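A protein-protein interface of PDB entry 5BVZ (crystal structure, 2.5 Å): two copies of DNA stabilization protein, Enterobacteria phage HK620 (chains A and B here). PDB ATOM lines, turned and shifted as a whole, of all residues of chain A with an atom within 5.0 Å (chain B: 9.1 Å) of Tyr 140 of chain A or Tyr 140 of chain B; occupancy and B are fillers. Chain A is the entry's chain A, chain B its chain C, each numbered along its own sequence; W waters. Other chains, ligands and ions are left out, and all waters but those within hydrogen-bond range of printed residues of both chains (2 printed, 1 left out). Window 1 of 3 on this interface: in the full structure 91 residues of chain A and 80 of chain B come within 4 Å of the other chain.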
ATOM      1  N   ILE A 136     -24.994  12.284 -19.233  1.00  0.00           N
ATOM      2  CA  ILE A 136     -23.738  12.389 -19.960  1.00  0.00           C
ATOM      3  C   ILE A 136     -23.092  13.760 -19.781  1.00  0.00           C
ATOM      4  O   ILE A 136     -21.898  13.846 -19.491  1.00  0.00           O
ATOM      5  CB  ILE A 136     -23.940  12.114 -21.461  1.00  0.00           C
ATOM      6  CG1 ILE A 136     -24.340  10.653 -21.679  1.00  0.00           C
ATOM      7  CG2 ILE A 136     -22.668  12.421 -22.235  1.00  0.00           C
ATOM      8  CD1 ILE A 136     -24.673  10.309 -23.121  1.00  0.00           C
ATOM      9  N   LYS A 137     -23.891  14.820 -19.897  1.00  0.00           N
ATOM     10  CA  LYS A 137     -23.387  16.191 -19.800  1.00  0.00           C
ATOM     11  C   LYS A 137     -22.636  16.441 -18.501  1.00  0.00           C
ATOM     12  O   LYS A 137     -21.613  17.121 -18.494  1.00  0.00           O
ATOM     13  CB  LYS A 137     -24.529  17.200 -19.954  1.00  0.00           C
ATOM     14  CG  LYS A 137     -24.751  17.619 -21.398  1.00  0.00           C
ATOM     15  CD  LYS A 137     -25.642  18.838 -21.533  1.00  0.00           C
ATOM     16  CE  LYS A 137     -27.045  18.547 -21.037  1.00  0.00           C
ATOM     17  NZ  LYS A 137     -27.950  19.709 -21.251  1.00  0.00           N
ATOM     18  N   SER A 138     -23.135  15.885 -17.405  1.00  0.00           N
ATOM     19  CA  SER A 138     -22.493  16.086 -16.113  1.00  0.00           C
ATOM     20  C   SER A 138     -21.291  15.161 -15.900  1.00  0.00           C
ATOM     21  O   SER A 138     -20.371  15.496 -15.152  1.00  0.00           O
ATOM     22  CB  SER A 138     -23.507  15.882 -14.987  1.00  0.00           C
ATOM     23  OG  SER A 138     -24.510  16.883 -15.020  1.00  0.00           O
ATOM     24  N   ASP A 139     -21.299  14.005 -16.558  1.00  0.00           N
ATOM     25  CA  ASP A 139     -20.286  12.984 -16.312  1.00  0.00           C
ATOM     26  C   ASP A 139     -19.070  13.015 -17.251  1.00  0.00           C
ATOM     27  O   ASP A 139     -18.040  12.405 -16.962  1.00  0.00           O
ATOM     28  CB  ASP A 139     -20.954  11.606 -16.404  1.00  0.00           C
ATOM     29  CG  ASP A 139     -20.091  10.490 -15.853  1.00  0.00           C
ATOM     30  OD1 ASP A 139     -19.456  10.683 -14.796  1.00  0.00           O
ATOM     31  OD2 ASP A 139     -20.039   9.418 -16.489  1.00  0.00           O
ATOM     32  N   TYR A 140     -19.180  13.728 -18.363  1.00  0.00           N
ATOM     33  CA  TYR A 140     -18.155  13.660 -19.402  1.00  0.00           C
ATOM     34  C   TYR A 140     -17.023  14.671 -19.234  1.00  0.00           C
ATOM     35  O   TYR A 140     -17.214  15.755 -18.685  1.00  0.00           O
ATOM     36  CB  TYR A 140     -18.805  13.803 -20.786  1.00  0.00           C
ATOM     37  CG  TYR A 140     -18.946  15.212 -21.317  1.00  0.00           C
ATOM     38  CD1 TYR A 140     -20.036  15.999 -20.975  1.00  0.00           C
ATOM     39  CD2 TYR A 140     -18.011  15.735 -22.203  1.00  0.00           C
ATOM     40  CE1 TYR A 140     -20.178  17.282 -21.476  1.00  0.00           C
ATOM     41  CE2 TYR A 140     -18.145  17.017 -22.712  1.00  0.00           C
ATOM     42  CZ  TYR A 140     -19.230  17.787 -22.346  1.00  0.00           C
ATOM     43  OH  TYR A 140     -19.363  19.066 -22.848  1.00  0.00           O
ATOM     44  N   VAL A 141     -15.832  14.289 -19.680  1.00  0.00           N
ATOM     45  CA  VAL A 141     -14.696  15.200 -19.688  1.00  0.00           C
ATOM     46  C   VAL A 141     -14.726  16.085 -20.929  1.00  0.00           C
ATOM     47  O   VAL A 141     -14.745  15.590 -22.056  1.00  0.00           O
ATOM     48  CB  VAL A 141     -13.356  14.454 -19.651  1.00  0.00           C
ATOM     49  CG1 VAL A 141     -12.197  15.451 -19.637  1.00  0.00           C
ATOM     50  CG2 VAL A 141     -13.298  13.521 -18.452  1.00  0.00           C
ATOM     51  N   SER A 142     -14.706  17.396 -20.699  1.00  0.00           N
ATOM     52  CA  SER A 142     -14.827  18.391 -21.760  1.00  0.00           C
ATOM     53  C   SER A 142     -13.476  18.900 -22.226  1.00  0.00           C
ATOM     54  O   SER A 142     -12.560  19.074 -21.422  1.00  0.00           O
ATOM     55  CB  SER A 142     -15.670  19.574 -21.288  1.00  0.00           C
ATOM     56  OG  SER A 142     -15.603  20.640 -22.218  1.00  0.00           O
ATOM     57  N   LYS A 143     -13.366  19.142 -23.530  1.00  0.00           N
ATOM     58  CA  LYS A 143     -12.139  19.661 -24.122  1.00  0.00           C
ATOM     59  C   LYS A 143     -12.038  21.191 -24.104  1.00  0.00           C
ATOM     60  O   LYS A 143     -10.944  21.731 -24.261  1.00  0.00           O
ATOM     61  CB  LYS A 143     -12.019  19.156 -25.563  1.00  0.00           C
ATOM     62  CG  LYS A 143     -11.951  17.632 -25.677  1.00  0.00           C
ATOM     63  CD  LYS A 143     -11.692  17.168 -27.105  1.00  0.00           C
ATOM     64  CE  LYS A 143     -12.865  17.507 -28.008  1.00  0.00           C
ATOM     65  NZ  LYS A 143     -12.643  17.053 -29.408  1.00  0.00           N
ATOM     66  N   GLN A 149     -10.352  19.108 -14.232  1.00  0.00           N
ATOM     67  CA  GLN A 149     -11.245  17.964 -14.303  1.00  0.00           C
ATOM     68  C   GLN A 149     -10.589  16.737 -13.673  1.00  0.00           C
ATOM     69  O   GLN A 149      -9.416  16.443 -13.921  1.00  0.00           O
ATOM     70  CB  GLN A 149     -11.631  17.690 -15.757  1.00  0.00           C
ATOM     71  CG  GLN A 149     -12.263  18.892 -16.447  1.00  0.00           C
ATOM     72  CD  GLN A 149     -12.677  18.598 -17.874  1.00  0.00           C
ATOM     73  OE1 GLN A 149     -13.753  18.053 -18.118  1.00  0.00           O
ATOM     74  NE2 GLN A 149     -11.828  18.964 -18.829  1.00  0.00           N
ATOM     75  N   ASP B 132     -28.241  19.287 -28.403  1.00  0.00           N
ATOM     76  CA  ASP B 132     -27.404  18.919 -27.261  1.00  0.00           C
ATOM     77  C   ASP B 132     -26.438  17.801 -27.622  1.00  0.00           C
ATOM     78  O   ASP B 132     -25.271  17.846 -27.245  1.00  0.00           O
ATOM     79  CB  ASP B 132     -28.263  18.491 -26.060  1.00  0.00           C
ATOM     80  CG  ASP B 132     -28.898  19.669 -25.332  1.00  0.00           C
ATOM     81  OD1 ASP B 132     -28.605  20.828 -25.694  1.00  0.00           O
ATOM     82  OD2 ASP B 132     -29.674  19.433 -24.380  1.00  0.00           O
ATOM     83  N   VAL B 133     -26.928  16.798 -28.343  1.00  0.00           N
ATOM     84  CA  VAL B 133     -26.082  15.701 -28.788  1.00  0.00           C
ATOM     85  C   VAL B 133     -24.975  16.221 -29.697  1.00  0.00           C
ATOM     86  O   VAL B 133     -23.814  15.824 -29.572  1.00  0.00           O
ATOM     87  CB  VAL B 133     -26.908  14.615 -29.519  1.00  0.00           C
ATOM     88  CG1 VAL B 133     -26.007  13.682 -30.320  1.00  0.00           C
ATOM     89  CG2 VAL B 133     -27.744  13.832 -28.517  1.00  0.00           C
ATOM     90  N   SER B 134     -25.339  17.144 -30.580  1.00  0.00           N
ATOM     91  CA  SER B 134     -24.385  17.775 -31.485  1.00  0.00           C
ATOM     92  C   SER B 134     -23.275  18.495 -30.719  1.00  0.00           C
ATOM     93  O   SER B 134     -22.097  18.391 -31.068  1.00  0.00           O
ATOM     94  CB  SER B 134     -25.105  18.755 -32.416  1.00  0.00           C
ATOM     95  OG  SER B 134     -24.196  19.352 -33.327  1.00  0.00           O
ATOM     96  N   ASP B 135     -23.668  19.249 -29.696  1.00  0.00           N
ATOM     97  CA  ASP B 135     -22.728  19.958 -28.835  1.00  0.00           C
ATOM     98  C   ASP B 135     -21.827  18.997 -28.054  1.00  0.00           C
ATOM     99  O   ASP B 135     -20.605  19.177 -28.004  1.00  0.00           O
ATOM    100  CB  ASP B 135     -23.487  20.870 -27.869  1.00  0.00           C
ATOM    101  CG  ASP B 135     -24.174  22.028 -28.574  1.00  0.00           C
ATOM    102  OD1 ASP B 135     -23.717  22.417 -29.671  1.00  0.00           O
ATOM    103  OD2 ASP B 135     -25.174  22.547 -28.032  1.00  0.00           O
ATOM    104  N   ILE B 136     -22.436  17.982 -27.443  1.00  0.00           N
ATOM    105  CA  ILE B 136     -21.691  16.985 -26.678  1.00  0.00           C
ATOM    106  C   ILE B 136     -20.699  16.246 -27.567  1.00  0.00           C
ATOM    107  O   ILE B 136     -19.546  16.036 -27.186  1.00  0.00           O
ATOM    108  CB  ILE B 136     -22.621  15.950 -26.017  1.00  0.00           C
ATOM    109  CG1 ILE B 136     -23.528  16.614 -24.980  1.00  0.00           C
ATOM    110  CG2 ILE B 136     -21.803  14.846 -25.366  1.00  0.00           C
ATOM    111  CD1 ILE B 136     -24.561  15.672 -24.382  1.00  0.00           C
ATOM    112  N   LYS B 137     -21.154  15.866 -28.758  1.00  0.00           N
ATOM    113  CA  LYS B 137     -20.329  15.107 -29.694  1.00  0.00           C
ATOM    114  C   LYS B 137     -19.014  15.803 -30.029  1.00  0.00           C
ATOM    115  O   LYS B 137     -17.969  15.158 -30.129  1.00  0.00           O
ATOM    116  CB  LYS B 137     -21.105  14.822 -30.982  1.00  0.00           C
ATOM    117  CG  LYS B 137     -21.874  13.512 -30.939  1.00  0.00           C
ATOM    118  CD  LYS B 137     -22.342  13.061 -32.316  1.00  0.00           C
ATOM    119  CE  LYS B 137     -23.340  14.028 -32.913  1.00  0.00           C
ATOM    120  NZ  LYS B 137     -23.851  13.524 -34.213  1.00  0.00           N
ATOM    121  N   SER B 138     -19.068  17.120 -30.187  1.00  0.00           N
ATOM    122  CA  SER B 138     -17.887  17.880 -30.560  1.00  0.00           C
ATOM    123  C   SER B 138     -16.966  18.176 -29.379  1.00  0.00           C
ATOM    124  O   SER B 138     -15.763  18.360 -29.554  1.00  0.00           O
ATOM    125  CB  SER B 138     -18.312  19.189 -31.222  1.00  0.00           C
ATOM    126  OG  SER B 138     -19.002  20.009 -30.294  1.00  0.00           O
ATOM    127  N   ASP B 139     -17.531  18.233 -28.179  1.00  0.00           N
ATOM    128  CA  ASP B 139     -16.762  18.649 -27.013  1.00  0.00           C
ATOM    129  C   ASP B 139     -16.167  17.511 -26.167  1.00  0.00           C
ATOM    130  O   ASP B 139     -15.292  17.755 -25.333  1.00  0.00           O
ATOM    131  CB  ASP B 139     -17.651  19.528 -26.132  1.00  0.00           C
ATOM    132  CG  ASP B 139     -16.867  20.308 -25.101  1.00  0.00           C
ATOM    133  OD1 ASP B 139     -15.777  20.819 -25.442  1.00  0.00           O
ATOM    134  OD2 ASP B 139     -17.356  20.427 -23.959  1.00  0.00           O
ATOM    135  N   TYR B 140     -16.614  16.274 -26.381  1.00  0.00           N
ATOM    136  CA  TYR B 140     -16.221  15.177 -25.483  1.00  0.00           C
ATOM    137  C   TYR B 140     -14.906  14.466 -25.850  1.00  0.00           C
ATOM    138  O   TYR B 140     -14.528  14.376 -27.021  1.00  0.00           O
ATOM    139  CB  TYR B 140     -17.359  14.149 -25.369  1.00  0.00           C
ATOM    140  CG  TYR B 140     -17.337  13.016 -26.369  1.00  0.00           C
ATOM    141  CD1 TYR B 140     -17.901  13.165 -27.629  1.00  0.00           C
ATOM    142  CD2 TYR B 140     -16.786  11.779 -26.037  1.00  0.00           C
ATOM    143  CE1 TYR B 140     -17.896  12.129 -28.541  1.00  0.00           C
ATOM    144  CE2 TYR B 140     -16.778  10.732 -26.943  1.00  0.00           C
ATOM    145  CZ  TYR B 140     -17.336  10.915 -28.193  1.00  0.00           C
ATOM    146  OH  TYR B 140     -17.337   9.887 -29.104  1.00  0.00           O
ATOM    147  N   VAL B 141     -14.214  13.966 -24.828  1.00  0.00           N
ATOM    148  CA  VAL B 141     -13.005  13.175 -25.040  1.00  0.00           C
ATOM    149  C   VAL B 141     -13.343  11.714 -25.343  1.00  0.00           C
ATOM    150  O   VAL B 141     -14.047  11.054 -24.577  1.00  0.00           O
ATOM    151  CB  VAL B 141     -12.075  13.236 -23.826  1.00  0.00           C
ATOM    152  CG1 VAL B 141     -10.803  12.458 -24.100  1.00  0.00           C
ATOM    153  CG2 VAL B 141     -11.755  14.684 -23.488  1.00  0.00           C
ATOM    154  N   SER B 142     -12.829  11.225 -26.469  1.00  0.00           N
ATOM    155  CA  SER B 142     -13.145   9.894 -26.973  1.00  0.00           C
ATOM    156  C   SER B 142     -12.119   8.843 -26.581  1.00  0.00           C
ATOM    157  O   SER B 142     -10.926   9.130 -26.506  1.00  0.00           O
ATOM    158  CB  SER B 142     -13.263   9.933 -28.498  1.00  0.00           C
ATOM    159  OG  SER B 142     -13.344   8.628 -29.049  1.00  0.00           O
ATOM    160  N   LYS B 143     -12.586   7.629 -26.304  1.00  0.00           N
ATOM    161  CA  LYS B 143     -11.669   6.535 -25.999  1.00  0.00           C
ATOM    162  C   LYS B 143     -11.200   5.805 -27.254  1.00  0.00           C
ATOM    163  O   LYS B 143     -10.248   5.036 -27.187  1.00  0.00           O
ATOM    164  CB  LYS B 143     -12.304   5.526 -25.039  1.00  0.00           C
ATOM    165  CG  LYS B 143     -12.688   6.098 -23.690  1.00  0.00           C
ATOM    166  CD  LYS B 143     -13.085   4.983 -22.739  1.00  0.00           C
ATOM    167  CE  LYS B 143     -14.333   4.268 -23.195  1.00  0.00           C
ATOM    168  NZ  LYS B 143     -14.692   3.185 -22.241  1.00  0.00           N
ATOM    169  N   THR B 144     -11.918   5.969 -28.367  1.00  0.00           N
ATOM    170  CA  THR B 144     -11.526   5.332 -29.629  1.00  0.00           C
ATOM    171  C   THR B 144     -10.846   6.232 -30.682  1.00  0.00           C
ATOM    172  O   THR B 144     -10.343   5.729 -31.683  1.00  0.00           O
ATOM    173  CB  THR B 144     -12.750   4.653 -30.291  1.00  0.00           C
ATOM    174  OG1 THR B 144     -13.807   5.607 -30.454  1.00  0.00           O
ATOM    175  CG2 THR B 144     -13.253   3.504 -29.426  1.00  0.00           C
ATOM    176  N   VAL B 145     -10.797   7.541 -30.454  1.00  0.00           N
ATOM    177  CA  VAL B 145     -10.142   8.458 -31.396  1.00  0.00           C
ATOM    178  C   VAL B 145      -8.619   8.322 -31.330  1.00  0.00           C
ATOM    179  O   VAL B 145      -8.053   8.321 -30.244  1.00  0.00           O
ATOM    180  CB  VAL B 145     -10.550   9.930 -31.123  1.00  0.00           C
ATOM    181  CG1 VAL B 145      -9.481  10.900 -31.586  1.00  0.00           C
ATOM    182  CG2 VAL B 145     -11.884  10.242 -31.773  1.00  0.00           C
ATOM    183  N   GLN B 149      -5.732  14.347 -28.491  1.00  0.00           N
ATOM    184  CA  GLN B 149      -6.821  15.114 -27.914  1.00  0.00           C
ATOM    185  C   GLN B 149      -6.272  16.050 -26.857  1.00  0.00           C
ATOM    186  O   GLN B 149      -5.471  15.654 -26.011  1.00  0.00           O
ATOM    187  CB  GLN B 149      -7.877  14.184 -27.309  1.00  0.00           C
ATOM    188  CG  GLN B 149      -8.456  13.173 -28.288  1.00  0.00           C
ATOM    189  CD  GLN B 149      -9.517  12.279 -27.655  1.00  0.00           C
ATOM    190  OE1 GLN B 149     -10.687  12.654 -27.555  1.00  0.00           O
ATOM    191  NE2 GLN B 149      -9.108  11.089 -27.226  1.00  0.00           N
ATOM    192  N   SER B 150      -6.726  17.294 -26.905  1.00  0.00           N
ATOM    193  CA  SER B 150      -6.206  18.321 -26.022  1.00  0.00           C
ATOM    194  C   SER B 150      -7.301  18.900 -25.135  1.00  0.00           C
ATOM    195  O   SER B 150      -8.396  19.230 -25.594  1.00  0.00           O
ATOM    196  CB  SER B 150      -5.530  19.429 -26.839  1.00  0.00           C
ATOM    197  OG  SER B 150      -5.090  20.489 -26.009  1.00  0.00           O
ATOM    198  N   LEU B 151      -6.984  19.009 -23.854  1.00  0.00           N
ATOM    199  CA  LEU B 151      -7.849  19.642 -22.883  1.00  0.00           C
ATOM    200  C   LEU B 151      -7.432  21.091 -22.680  1.00  0.00           C
ATOM    201  O   LEU B 151      -6.252  21.432 -22.772  1.00  0.00           O
ATOM    202  CB  LEU B 151      -7.801  18.886 -21.556  1.00  0.00           C
ATOM    203  CG  LEU B 151      -8.214  17.419 -21.637  1.00  0.00           C
ATOM    204  CD1 LEU B 151      -8.189  16.784 -20.262  1.00  0.00           C
ATOM    205  CD2 LEU B 151      -9.597  17.318 -22.251  1.00  0.00           C
ATOM    206  N   SER B 153      -8.016  22.337 -19.891  1.00  0.00           N
ATOM    207  CA  SER B 153      -7.985  22.304 -18.431  1.00  0.00           C
ATOM    208  C   SER B 153      -6.876  21.423 -17.867  1.00  0.00           C
ATOM    209  O   SER B 153      -6.312  20.602 -18.585  1.00  0.00           O
ATOM    210  CB  SER B 153      -9.329  21.800 -17.893  1.00  0.00           C
ATOM    211  OG  SER B 153      -9.516  20.430 -18.210  1.00  0.00           O
HETATM  212  O   HOH W   1     -10.908  20.982 -21.104  1.00  0.00           O
HETATM  213  O   HOH W   2     -15.480  12.447 -22.847  1.00  0.00           O
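Water W1 lies within hydrogen-bond range of the backbone carbonyl oxygen (O) of Ser 142 of chain A, the side-chain amide nitrogen (NE2) of Gln 149 of chain A, the backbone carbonyl oxygen (O) of Lys 143 of chain A and the side-chain hydroxyl (OG) of Ser 153 of chain B. Water W2 bridges O of Val 141 of chain B (2.6 Å) and O of Val 141 of chain A (3.3 Å).
Among the printed residues, merely in contact across the chains: Lys 137 of chain A with Ile 136 of chain B, Tyr 140 of chain A with Tyr 140 of chain B, Val 141 of chain A with Asp 139 of chain B, Val 141 of chain A with Tyr 140 of chain B, Ser 142 of chain A with Leu 151 of chain B, Lys 143 of chain A with Tyr 140 of chain B, Lys 143 of chain A with Val 141 of chain B, Lys 143 of chain A with Ser 150 of chain B and Lys 143 of chain A with Leu 151 of chain B.
Of the 18 printed residues of chain B, 9 touch a printed residue of chain A. Printed residues of chain B that touch a printed residue of chain A: Asp 132, Ile 136, Ser 138, Asp 139, Tyr 140, Val 141, Ser 150, Leu 151 and Ser 153. Hydrophobic or aromatic side chains of chain A within 4 Å of the printed part of chain B: Tyr 140 and Val 141. Among the printed residues, 16 pairs touch across the chains. Among the printed residues, Asp or Glu carboxylates within 4 Å of a Lys or Arg side-chain nitrogen of the other chain: Lys 137 of chain A with Asp 132 of chain B (3.6 Å).
Lys 137 of chain A touches Ile 136 of chain B, but with the chains exchanged Ile 136 of chain A does not touch Lys 137 of chain B (7.5 Å). Tyr 140 of chain A touches Asp 139 of chain B, but with the chains exchanged Asp 139 of chain A does not touch Tyr 140 of chain B (8.4 Å). Val 141 of chain A touches Tyr 140 of chain B, but with the chains exchanged Tyr 140 of chain A does not touch Val 141 of chain B (4.9 Å). Lys 143 of chain A touches Asp 139 of chain B, but with the chains exchanged Asp 139 of chain A does not touch Lys 143 of chain B (10.0 Å). Of the 16 pairs that touch across the chains among the printed residues, 2 have their exchanged pair printed and touching as well.
The side-chain hydroxyl of Ser 142 of chain A lies within hydrogen-bond range of the side-chain carboxylate of Asp 139 of chain B (2.5 Å). N of Val 141 of chain B is in hydrogen-bond range of O of Val 141 of chain A. The side-chain hydroxyl (OH) of Tyr 140 of chain A lies within hydrogen-bond range of the side-chain carboxylate (OD2) of Asp 139 of chain B (2.7 Å). The backbone carbonyl oxygen (O) of Ser 138 of chain B lies within hydrogen-bond range of the side-chain amino group (NZ) of Lys 143 of chain A. The side-chain amide nitrogen of Gln 149 of chain A sits at hydrogen-bond distance from the side-chain hydroxyl of Ser 153 of chain B, at 2.8 Å. OD2 of Asp 132 of chain B lies within salt-bridge range of NZ of Lys 137 of chain A, 3.6 Å away. The backbone NH of Lys 143 of chain A lies within hydrogen-bond range of the backbone carbonyl oxygen of Asp 139 of chain B, at 3.0 Å.
Of the printed residues of chain B, Lys 137 of chain A touches Asp 132 and Ile 136. No residue of chain B comes within 4 Å of Asp 139 of chain A. Val 141 of chain A touches just these residues of chain B: Asp 139 (3.97 Å), Tyr 140 (3.8 Å) and Val 141 (3.3 Å). Lys 137 of chain B touches none of the printed residues of chain A. Of the printed residues of chain A, Tyr 140 of chain B touches Tyr 140, Val 141 and Lys 143. Gln 149 of chain B touches none of the printed residues of chain A. Of the printed residues of chain A, Ser 150 of chain B touches Lys 143. The nearest residue of chain B that does not touch Tyr 140 of chain A is Ile 136 of chain B (4.8 Å).
The side-chain hydroxyl of Ser 138 of chain B lies within hydrogen-bond range of the backbone carbonyl oxygen of Asp 135 of chain B. The backbone carbonyl oxygen (O) of Ser 142 of chain A lies within hydrogen-bond range of the side-chain amide nitrogen (NE2) of Gln 149 of chain A, at 2.7 Å.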
